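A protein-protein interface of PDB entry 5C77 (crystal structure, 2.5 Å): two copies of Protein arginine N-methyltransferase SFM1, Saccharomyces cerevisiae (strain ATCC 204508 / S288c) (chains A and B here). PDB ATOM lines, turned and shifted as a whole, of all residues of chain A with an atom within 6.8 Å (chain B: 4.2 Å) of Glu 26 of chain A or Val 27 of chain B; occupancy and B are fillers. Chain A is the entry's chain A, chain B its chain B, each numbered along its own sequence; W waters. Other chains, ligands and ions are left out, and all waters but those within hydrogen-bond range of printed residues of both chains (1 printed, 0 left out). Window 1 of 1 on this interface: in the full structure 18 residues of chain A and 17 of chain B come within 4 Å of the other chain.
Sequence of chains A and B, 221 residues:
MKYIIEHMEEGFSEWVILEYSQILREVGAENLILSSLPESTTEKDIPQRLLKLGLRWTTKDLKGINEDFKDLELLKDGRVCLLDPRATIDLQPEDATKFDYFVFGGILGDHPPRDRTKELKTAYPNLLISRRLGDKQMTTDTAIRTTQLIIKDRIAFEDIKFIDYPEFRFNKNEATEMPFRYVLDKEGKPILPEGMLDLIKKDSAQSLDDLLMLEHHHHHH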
ATOM      1  N   SER A  21      -7.787 -22.413   0.543  1.00  0.00           N
ATOM      2  CA  SER A  21      -6.626 -21.585   0.895  1.00  0.00           C
ATOM      3  C   SER A  21      -7.035 -20.356   1.686  1.00  0.00           C
ATOM      4  O   SER A  21      -6.429 -20.023   2.698  1.00  0.00           O
ATOM      5  CB  SER A  21      -5.897 -21.105  -0.363  1.00  0.00           C
ATOM      6  OG  SER A  21      -4.877 -21.999  -0.759  1.00  0.00           O
ATOM      7  N   GLN A  22      -8.070 -19.683   1.187  1.00  0.00           N
ATOM      8  CA  GLN A  22      -8.562 -18.451   1.781  1.00  0.00           C
ATOM      9  C   GLN A  22      -9.149 -18.748   3.156  1.00  0.00           C
ATOM     10  O   GLN A  22      -8.871 -18.041   4.132  1.00  0.00           O
ATOM     11  CB  GLN A  22      -9.616 -17.825   0.862  1.00  0.00           C
ATOM     12  CG  GLN A  22     -10.028 -16.423   1.221  1.00  0.00           C
ATOM     13  CD  GLN A  22      -8.885 -15.422   1.135  1.00  0.00           C
ATOM     14  OE1 GLN A  22      -7.892 -15.629   0.432  1.00  0.00           O
ATOM     15  NE2 GLN A  22      -9.023 -14.322   1.867  1.00  0.00           N
ATOM     16  N   ILE A  23      -9.955 -19.802   3.225  1.00  0.00           N
ATOM     17  CA  ILE A  23     -10.528 -20.229   4.485  1.00  0.00           C
ATOM     18  C   ILE A  23      -9.423 -20.499   5.516  1.00  0.00           C
ATOM     19  O   ILE A  23      -9.486 -20.011   6.639  1.00  0.00           O
ATOM     20  CB  ILE A  23     -11.430 -21.470   4.300  1.00  0.00           C
ATOM     21  CG1 ILE A  23     -12.715 -21.075   3.568  1.00  0.00           C
ATOM     22  CG2 ILE A  23     -11.764 -22.096   5.639  1.00  0.00           C
ATOM     23  CD1 ILE A  23     -13.440 -22.237   2.936  1.00  0.00           C
ATOM     24  N   LEU A  24      -8.407 -21.252   5.115  1.00  0.00           N
ATOM     25  CA  LEU A  24      -7.296 -21.574   5.991  1.00  0.00           C
ATOM     26  C   LEU A  24      -6.618 -20.327   6.551  1.00  0.00           C
ATOM     27  O   LEU A  24      -6.393 -20.231   7.754  1.00  0.00           O
ATOM     28  CB  LEU A  24      -6.276 -22.447   5.261  1.00  0.00           C
ATOM     29  CG  LEU A  24      -6.642 -23.924   5.133  1.00  0.00           C
ATOM     30  CD1 LEU A  24      -5.799 -24.612   4.073  1.00  0.00           C
ATOM     31  CD2 LEU A  24      -6.510 -24.625   6.482  1.00  0.00           C
ATOM     32  N   ARG A  25      -6.311 -19.363   5.690  1.00  0.00           N
ATOM     33  CA  ARG A  25      -5.642 -18.154   6.150  1.00  0.00           C
ATOM     34  C   ARG A  25      -6.513 -17.221   7.009  1.00  0.00           C
ATOM     35  O   ARG A  25      -5.991 -16.359   7.704  1.00  0.00           O
ATOM     36  CB  ARG A  25      -4.972 -17.406   4.990  1.00  0.00           C
ATOM     37  CG  ARG A  25      -5.869 -17.090   3.822  1.00  0.00           C
ATOM     38  CD  ARG A  25      -5.150 -16.240   2.776  1.00  0.00           C
ATOM     39  NE  ARG A  25      -4.182 -16.973   1.965  1.00  0.00           N
ATOM     40  CZ  ARG A  25      -4.439 -17.443   0.743  1.00  0.00           C
ATOM     41  NH1 ARG A  25      -5.644 -17.272   0.199  1.00  0.00           N
ATOM     42  NH2 ARG A  25      -3.494 -18.091   0.066  1.00  0.00           N
ATOM     43  N   GLU A  26      -7.828 -17.418   6.998  1.00  0.00           N
ATOM     44  CA  GLU A  26      -8.709 -16.566   7.784  1.00  0.00           C
ATOM     45  C   GLU A  26      -9.149 -17.148   9.122  1.00  0.00           C
ATOM     46  O   GLU A  26      -9.471 -16.396  10.034  1.00  0.00           O
ATOM     47  CB  GLU A  26      -9.922 -16.146   6.972  1.00  0.00           C
ATOM     48  CG  GLU A  26      -9.553 -15.381   5.727  1.00  0.00           C
ATOM     49  CD  GLU A  26     -10.755 -14.742   5.059  1.00  0.00           C
ATOM     50  OE1 GLU A  26     -10.713 -14.533   3.820  1.00  0.00           O
ATOM     51  OE2 GLU A  26     -11.744 -14.439   5.773  1.00  0.00           O
ATOM     52  N   VAL A  27      -9.168 -18.472   9.248  1.00  0.00           N
ATOM     53  CA  VAL A  27      -9.568 -19.092  10.516  1.00  0.00           C
ATOM     54  C   VAL A  27      -8.382 -19.768  11.208  1.00  0.00           C
ATOM     55  O   VAL A  27      -8.395 -19.995  12.429  1.00  0.00           O
ATOM     56  CB  VAL A  27     -10.750 -20.103  10.355  1.00  0.00           C
ATOM     57  CG1 VAL A  27     -11.924 -19.435   9.670  1.00  0.00           C
ATOM     58  CG2 VAL A  27     -10.319 -21.352   9.597  1.00  0.00           C
ATOM     59  N   GLY A  28      -7.347 -20.061  10.422  1.00  0.00           N
ATOM     60  CA  GLY A  28      -6.189 -20.764  10.926  1.00  0.00           C
ATOM     61  C   GLY A  28      -6.381 -22.261  10.823  1.00  0.00           C
ATOM     62  O   GLY A  28      -7.463 -22.775  11.089  1.00  0.00           O
ATOM     63  N   ALA A  29      -5.307 -22.953  10.463  1.00  0.00           N
ATOM     64  CA  ALA A  29      -5.309 -24.390  10.228  1.00  0.00           C
ATOM     65  C   ALA A  29      -5.816 -25.269  11.378  1.00  0.00           C
ATOM     66  O   ALA A  29      -6.353 -26.349  11.120  1.00  0.00           O
ATOM     67  CB  ALA A  29      -3.926 -24.834   9.809  1.00  0.00           C
ATOM     68  N   GLU A  30      -5.630 -24.834  12.629  1.00  0.00           N
ATOM     69  CA  GLU A  30      -6.101 -25.597  13.793  1.00  0.00           C
ATOM     70  C   GLU A  30      -7.627 -25.595  13.930  1.00  0.00           C
ATOM     71  O   GLU A  30      -8.191 -26.364  14.708  1.00  0.00           O
ATOM     72  CB  GLU A  30      -5.497 -25.059  15.097  1.00  0.00           C
ATOM     73  CG  GLU A  30      -4.017 -25.360  15.294  1.00  0.00           C
ATOM     74  CD  GLU A  30      -3.685 -26.843  15.130  1.00  0.00           C
ATOM     75  OE1 GLU A  30      -4.012 -27.621  16.055  1.00  0.00           O
ATOM     76  OE2 GLU A  30      -3.101 -27.231  14.083  1.00  0.00           O
ATOM     77  N   ASN A  31      -8.292 -24.729  13.177  1.00  0.00           N
ATOM     78  CA  ASN A  31      -9.718 -24.514  13.351  1.00  0.00           C
ATOM     79  C   ASN A  31     -10.584 -25.067  12.219  1.00  0.00           C
ATOM     80  O   ASN A  31     -11.809 -25.076  12.311  1.00  0.00           O
ATOM     81  CB  ASN A  31      -9.975 -23.030  13.561  1.00  0.00           C
ATOM     82  CG  ASN A  31      -9.330 -22.525  14.826  1.00  0.00           C
ATOM     83  OD1 ASN A  31      -9.583 -23.056  15.903  1.00  0.00           O
ATOM     84  ND2 ASN A  31      -8.459 -21.527  14.701  1.00  0.00           N
ATOM     85  N   ASP A 141     -16.341 -20.117   1.362  1.00  0.00           N
ATOM     86  CA  ASP A 141     -15.491 -19.153   2.061  1.00  0.00           C
ATOM     87  C   ASP A 141     -16.282 -17.949   2.548  1.00  0.00           C
ATOM     88  O   ASP A 141     -15.971 -17.372   3.599  1.00  0.00           O
ATOM     89  CB  ASP A 141     -14.322 -18.709   1.184  1.00  0.00           C
ATOM     90  CG  ASP A 141     -14.773 -17.978  -0.075  1.00  0.00           C
ATOM     91  OD1 ASP A 141     -15.057 -18.655  -1.104  1.00  0.00           O
ATOM     92  OD2 ASP A 141     -14.820 -16.723  -0.035  1.00  0.00           O
ATOM     93  N   ILE A 144     -18.291 -19.296   5.526  1.00  0.00           N
ATOM     94  CA  ILE A 144     -17.428 -19.353   6.686  1.00  0.00           C
ATOM     95  C   ILE A 144     -17.120 -17.955   7.235  1.00  0.00           C
ATOM     96  O   ILE A 144     -17.128 -17.746   8.447  1.00  0.00           O
ATOM     97  CB  ILE A 144     -16.172 -20.181   6.387  1.00  0.00           C
ATOM     98  CG1 ILE A 144     -16.583 -21.644   6.230  1.00  0.00           C
ATOM     99  CG2 ILE A 144     -15.115 -20.026   7.500  1.00  0.00           C
ATOM    100  CD1 ILE A 144     -15.453 -22.555   5.949  1.00  0.00           C
ATOM    101  N   ARG A 145     -16.886 -17.000   6.342  1.00  0.00           N
ATOM    102  CA  ARG A 145     -16.591 -15.634   6.753  1.00  0.00           C
ATOM    103  C   ARG A 145     -17.774 -15.065   7.530  1.00  0.00           C
ATOM    104  O   ARG A 145     -17.615 -14.393   8.555  1.00  0.00           O
ATOM    105  CB  ARG A 145     -16.294 -14.784   5.524  1.00  0.00           C
ATOM    106  CG  ARG A 145     -15.911 -13.341   5.815  1.00  0.00           C
ATOM    107  CD  ARG A 145     -15.129 -12.722   4.648  1.00  0.00           C
ATOM    108  NE  ARG A 145     -15.319 -13.456   3.400  1.00  0.00           N
ATOM    109  CZ  ARG A 145     -14.389 -14.214   2.821  1.00  0.00           C
ATOM    110  NH1 ARG A 145     -13.190 -14.332   3.372  1.00  0.00           N
ATOM    111  NH2 ARG A 145     -14.653 -14.852   1.684  1.00  0.00           N
ATOM    112  N   GLN A 148     -18.211 -16.686  10.929  1.00  0.00           N
ATOM    113  CA  GLN A 148     -17.210 -16.086  11.795  1.00  0.00           C
ATOM    114  C   GLN A 148     -17.598 -14.688  12.269  1.00  0.00           C
ATOM    115  O   GLN A 148     -17.331 -14.321  13.414  1.00  0.00           O
ATOM    116  CB  GLN A 148     -15.867 -16.036  11.074  1.00  0.00           C
ATOM    117  CG  GLN A 148     -14.730 -15.646  11.957  1.00  0.00           C
ATOM    118  CD  GLN A 148     -13.407 -15.801  11.262  1.00  0.00           C
ATOM    119  OE1 GLN A 148     -12.539 -16.558  11.713  1.00  0.00           O
ATOM    120  NE2 GLN A 148     -13.237 -15.089  10.149  1.00  0.00           N
ATOM    121  N   ILE A 191     -15.637  -9.547  -1.266  1.00  0.00           N
ATOM    122  CA  ILE A 191     -14.479 -10.322  -0.858  1.00  0.00           C
ATOM    123  C   ILE A 191     -14.492 -11.691  -1.510  1.00  0.00           C
ATOM    124  O   ILE A 191     -15.376 -12.501  -1.254  1.00  0.00           O
ATOM    125  CB  ILE A 191     -14.424 -10.522   0.670  1.00  0.00           C
ATOM    126  CG1 ILE A 191     -14.535  -9.180   1.396  1.00  0.00           C
ATOM    127  CG2 ILE A 191     -13.144 -11.238   1.058  1.00  0.00           C
ATOM    128  CD1 ILE A 191     -14.693  -9.300   2.889  1.00  0.00           C
ATOM    129  N   LEU A 192     -13.500 -11.934  -2.354  1.00  0.00           N
ATOM    130  CA  LEU A 192     -13.294 -13.231  -2.973  1.00  0.00           C
ATOM    131  C   LEU A 192     -11.960 -13.775  -2.484  1.00  0.00           C
ATOM    132  O   LEU A 192     -11.115 -13.009  -2.011  1.00  0.00           O
ATOM    133  CB  LEU A 192     -13.284 -13.105  -4.503  1.00  0.00           C
ATOM    134  CG  LEU A 192     -14.635 -13.203  -5.224  1.00  0.00           C
ATOM    135  CD1 LEU A 192     -15.555 -12.056  -4.839  1.00  0.00           C
ATOM    136  CD2 LEU A 192     -14.441 -13.249  -6.730  1.00  0.00           C
ATOM    137  N   PRO A 193     -11.771 -15.102  -2.572  1.00  0.00           N
ATOM    138  CA  PRO A 193     -10.470 -15.664  -2.209  1.00  0.00           C
ATOM    139  C   PRO A 193      -9.392 -15.107  -3.107  1.00  0.00           C
ATOM    140  O   PRO A 193      -9.684 -14.683  -4.221  1.00  0.00           O
ATOM    141  CB  PRO A 193     -10.656 -17.159  -2.468  1.00  0.00           C
ATOM    142  CG  PRO A 193     -12.107 -17.384  -2.227  1.00  0.00           C
ATOM    143  CD  PRO A 193     -12.778 -16.153  -2.789  1.00  0.00           C
ATOM    144  N   TYR B   3      -3.909  -8.900  14.844  1.00  0.00           N
ATOM    145  CA  TYR B   3      -2.806  -8.838  15.799  1.00  0.00           C
ATOM    146  C   TYR B   3      -1.521  -8.357  15.139  1.00  0.00           C
ATOM    147  O   TYR B   3      -1.164  -8.801  14.043  1.00  0.00           O
ATOM    148  CB  TYR B   3      -2.547 -10.211  16.415  1.00  0.00           C
ATOM    149  CG  TYR B   3      -3.756 -10.879  17.007  1.00  0.00           C
ATOM    150  CD1 TYR B   3      -4.585 -11.673  16.221  1.00  0.00           C
ATOM    151  CD2 TYR B   3      -4.073 -10.725  18.349  1.00  0.00           C
ATOM    152  CE1 TYR B   3      -5.689 -12.295  16.753  1.00  0.00           C
ATOM    153  CE2 TYR B   3      -5.184 -11.347  18.894  1.00  0.00           C
ATOM    154  CZ  TYR B   3      -5.984 -12.131  18.087  1.00  0.00           C
ATOM    155  OH  TYR B   3      -7.090 -12.756  18.608  1.00  0.00           O
ATOM    156  N   ILE B  23       0.655 -19.576  16.781  1.00  0.00           N
ATOM    157  CA  ILE B  23      -0.167 -18.384  16.601  1.00  0.00           C
ATOM    158  C   ILE B  23      -0.815 -18.357  15.215  1.00  0.00           C
ATOM    159  O   ILE B  23      -2.021 -18.147  15.092  1.00  0.00           O
ATOM    160  CB  ILE B  23       0.673 -17.108  16.847  1.00  0.00           C
ATOM    161  CG1 ILE B  23       1.134 -17.069  18.312  1.00  0.00           C
ATOM    162  CG2 ILE B  23      -0.106 -15.858  16.471  1.00  0.00           C
ATOM    163  CD1 ILE B  23       2.207 -16.072  18.609  1.00  0.00           C
ATOM    164  N   LEU B  24      -0.015 -18.587  14.182  1.00  0.00           N
ATOM    165  CA  LEU B  24      -0.510 -18.588  12.813  1.00  0.00           C
ATOM    166  C   LEU B  24      -1.596 -19.624  12.622  1.00  0.00           C
ATOM    167  O   LEU B  24      -2.565 -19.363  11.935  1.00  0.00           O
ATOM    168  CB  LEU B  24       0.615 -18.854  11.818  1.00  0.00           C
ATOM    169  CG  LEU B  24       1.544 -17.704  11.435  1.00  0.00           C
ATOM    170  CD1 LEU B  24       2.631 -18.214  10.489  1.00  0.00           C
ATOM    171  CD2 LEU B  24       0.769 -16.542  10.814  1.00  0.00           C
ATOM    172  N   ARG B  25      -1.440 -20.791  13.242  1.00  0.00           N
ATOM    173  CA  ARG B  25      -2.402 -21.877  13.057  1.00  0.00           C
ATOM    174  C   ARG B  25      -3.704 -21.651  13.840  1.00  0.00           C
ATOM    175  O   ARG B  25      -4.750 -22.214  13.505  1.00  0.00           O
ATOM    176  CB  ARG B  25      -1.772 -23.237  13.390  1.00  0.00           C
ATOM    177  CG  ARG B  25      -0.611 -23.637  12.448  1.00  0.00           C
ATOM    178  CD  ARG B  25      -0.121 -25.076  12.665  1.00  0.00           C
ATOM    179  NE  ARG B  25       0.314 -25.306  14.039  1.00  0.00           N
ATOM    180  CZ  ARG B  25       1.582 -25.298  14.439  1.00  0.00           C
ATOM    181  NH1 ARG B  25       2.558 -25.098  13.563  1.00  0.00           N
ATOM    182  NH2 ARG B  25       1.879 -25.501  15.712  1.00  0.00           N
ATOM    183  N   GLU B  26      -3.635 -20.801  14.864  1.00  0.00           N
ATOM    184  CA  GLU B  26      -4.789 -20.528  15.721  1.00  0.00           C
ATOM    185  C   GLU B  26      -5.605 -19.281  15.358  1.00  0.00           C
ATOM    186  O   GLU B  26      -6.765 -19.180  15.739  1.00  0.00           O
ATOM    187  CB  GLU B  26      -4.359 -20.444  17.188  1.00  0.00           C
ATOM    188  CG  GLU B  26      -3.850 -21.741  17.757  1.00  0.00           C
ATOM    189  CD  GLU B  26      -3.896 -21.768  19.277  1.00  0.00           C
ATOM    190  OE1 GLU B  26      -4.715 -21.022  19.866  1.00  0.00           O
ATOM    191  OE2 GLU B  26      -3.108 -22.535  19.885  1.00  0.00           O
ATOM    192  N   VAL B  27      -5.002 -18.324  14.662  1.00  0.00           N
ATOM    193  CA  VAL B  27      -5.699 -17.079  14.326  1.00  0.00           C
ATOM    194  C   VAL B  27      -5.795 -16.890  12.813  1.00  0.00           C
ATOM    195  O   VAL B  27      -6.655 -16.165  12.315  1.00  0.00           O
ATOM    196  CB  VAL B  27      -5.048 -15.827  15.001  1.00  0.00           C
ATOM    197  CG1 VAL B  27      -4.927 -16.035  16.503  1.00  0.00           C
ATOM    198  CG2 VAL B  27      -3.673 -15.507  14.400  1.00  0.00           C
ATOM    199  N   GLY B  28      -4.922 -17.564  12.077  1.00  0.00           N
ATOM    200  CA  GLY B  28      -4.905 -17.411  10.639  1.00  0.00           C
ATOM    201  C   GLY B  28      -3.910 -16.356  10.213  1.00  0.00           C
ATOM    202  O   GLY B  28      -3.844 -15.274  10.793  1.00  0.00           O
ATOM    203  N   ASN B  31      -4.666 -12.638   9.783  1.00  0.00           N
ATOM    204  CA  ASN B  31      -4.976 -11.831  10.955  1.00  0.00           C
ATOM    205  C   ASN B  31      -3.756 -11.481  11.809  1.00  0.00           C
ATOM    206  O   ASN B  31      -3.884 -11.027  12.941  1.00  0.00           O
ATOM    207  CB  ASN B  31      -6.002 -12.575  11.807  1.00  0.00           C
ATOM    208  CG  ASN B  31      -7.228 -12.995  11.004  1.00  0.00           C
ATOM    209  OD1 ASN B  31      -7.850 -12.170  10.339  1.00  0.00           O
ATOM    210  ND2 ASN B  31      -7.564 -14.281  11.049  1.00  0.00           N
ATOM    211  N   ILE B 144      -1.712 -13.839  23.064  1.00  0.00           N
ATOM    212  CA  ILE B 144      -2.627 -13.829  21.925  1.00  0.00           C
ATOM    213  C   ILE B 144      -3.833 -14.759  22.149  1.00  0.00           C
ATOM    214  O   ILE B 144      -4.981 -14.390  21.857  1.00  0.00           O
ATOM    215  CB  ILE B 144      -1.893 -14.161  20.614  1.00  0.00           C
ATOM    216  CG1 ILE B 144      -1.037 -12.971  20.190  1.00  0.00           C
ATOM    217  CG2 ILE B 144      -2.874 -14.490  19.516  1.00  0.00           C
ATOM    218  CD1 ILE B 144      -0.244 -13.204  18.954  1.00  0.00           C
ATOM    219  N   GLN B 148      -7.706 -13.395  22.337  1.00  0.00           N
ATOM    220  CA  GLN B 148      -8.714 -14.038  21.506  1.00  0.00           C
ATOM    221  C   GLN B 148      -9.942 -14.498  22.312  1.00  0.00           C
ATOM    222  O   GLN B 148     -11.077 -14.258  21.906  1.00  0.00           O
ATOM    223  CB  GLN B 148      -8.074 -15.209  20.756  1.00  0.00           C
ATOM    224  CG  GLN B 148      -8.990 -15.933  19.812  1.00  0.00           C
ATOM    225  CD  GLN B 148      -8.419 -16.013  18.405  1.00  0.00           C
ATOM    226  OE1 GLN B 148      -8.390 -15.017  17.667  1.00  0.00           O
ATOM    227  NE2 GLN B 148      -7.972 -17.206  18.020  1.00  0.00           N
HETATM  228  O   HOH W   1      -2.899 -21.237   9.850  1.00  0.00           O
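The backbone carbonyl oxygen of Glu 26 of chain A sits at hydrogen-bond distance from the side-chain amide nitrogen of Asn 31 of chain B, at 3.0 Å.
N of Ala 29 of chain A sits at hydrogen-bond distance from O of Arg 25 of chain B, 3.2 Å away.
OE2 of Glu 30 of chain A is in salt-bridge range of NE of Arg 25 of chain B.
O of Glu 26 of chain B sits at hydrogen-bond distance from ND2 of Asn 31 of chain A, at 3.1 Å.
The guanidinium group (NH1) of Arg 25 of chain A sits at hydrogen-bond distance from the side-chain amide oxygen (OE1) of Gln 22 of chain A (2.8 Å).
NE2 of Gln 22 of chain A lies within hydrogen-bond range of OE1 of Glu 26 of chain A (2.6 Å).
The guanidinium group (NH1) of Arg 145 of chain A lies within salt-bridge range of the side-chain carboxylate (OE1) of Glu 26 of chain A (2.5 Å).
The backbone NH (N) of Tyr 3 of chain B lies within hydrogen-bond range of the backbone carbonyl oxygen (O) of Asn 31 of chain B (2.9 Å).
O of Glu 26 of chain B is in hydrogen-bond range of NE2 of Gln 148 of chain B (3.2 Å).
O of Val 27 of chain B is in hydrogen-bond range of ND2 of Asn 31 of chain B (2.4 Å).
O of Arg 25 of chain A touches C of Gly 28 of chain B, at 3.3 Å.
O of Glu 26 of chain A touches O of Val 27 of chain B, 3.6 Å away.
O of Val 27 of chain A touches O of Glu 26 of chain B (3.8 Å).
C of Gly 28 of chain A touches O of Arg 25 of chain B, 3.1 Å away.
Gly 28 of chain A touches Gly 28 of chain B.
Asn 31 of chain A touches Arg 25 of chain B.
Printed residues of chain B within 4 Å of Glu 30 of chain A: Arg 25 (2.9 Å).
Arg 145 of chain A touches none of the printed residues of chain B.
Leu 192 of chain A touches none of the printed residues of chain B.
Of the printed residues of chain A, Gly 28 of chain B touches Arg 25 (3.3 Å) and Gly 28 (3.6 Å).
The nearest printed residue of chain B that does not touch Glu 26 of chain A is Gly 28 of chain B (4.5 Å).
The nearest residue of chain A that does not touch Val 27 of chain B is Val 27 of chain A (4.1 Å).
The nearest printed residue of chain A that does not touch Gly 28 of chain B is Val 27 of chain A (4.2 Å).
Printed residues of chain A that touch a printed residue of chain B: Arg 25, Glu 26, Val 27, Gly 28, Ala 29, Glu 30 and Asn 31.
Printed residues of chain B that touch a printed residue of chain A: Arg 25, Glu 26, Val 27, Gly 28 and Asn 31.
Among the printed residues, Asp or Glu carboxylates within 4 Å of a Lys or Arg side-chain nitrogen of the other chain: Glu 30 of chain A with Arg 25 of chain B (3.9 Å).
Arg 25 of chain A touches Gly 28 of chain B, and with the chains exchanged Gly 28 of chain A touches Arg 25 of chain B.
Glu 26 of chain A touches Asn 31 of chain B, and with the chains exchanged Asn 31 of chain A touches Glu 26 of chain B.
Gly 28 of chain A touches its own counterpart, Gly 28 of chain B.
Asn 31 of chain A touches Arg 25 of chain B, but with the chains exchanged Arg 25 of chain A does not touch Asn 31 of chain B (4.2 Å).
Of the 10 pairs that touch across the chains among the printed residues, 7 have their exchanged pair printed and touching as well.
Water W1 lies within hydrogen-bond range of the backbone carbonyl oxygen of Leu 24 of chain B and the backbone NH of Ala 29 of chain A.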
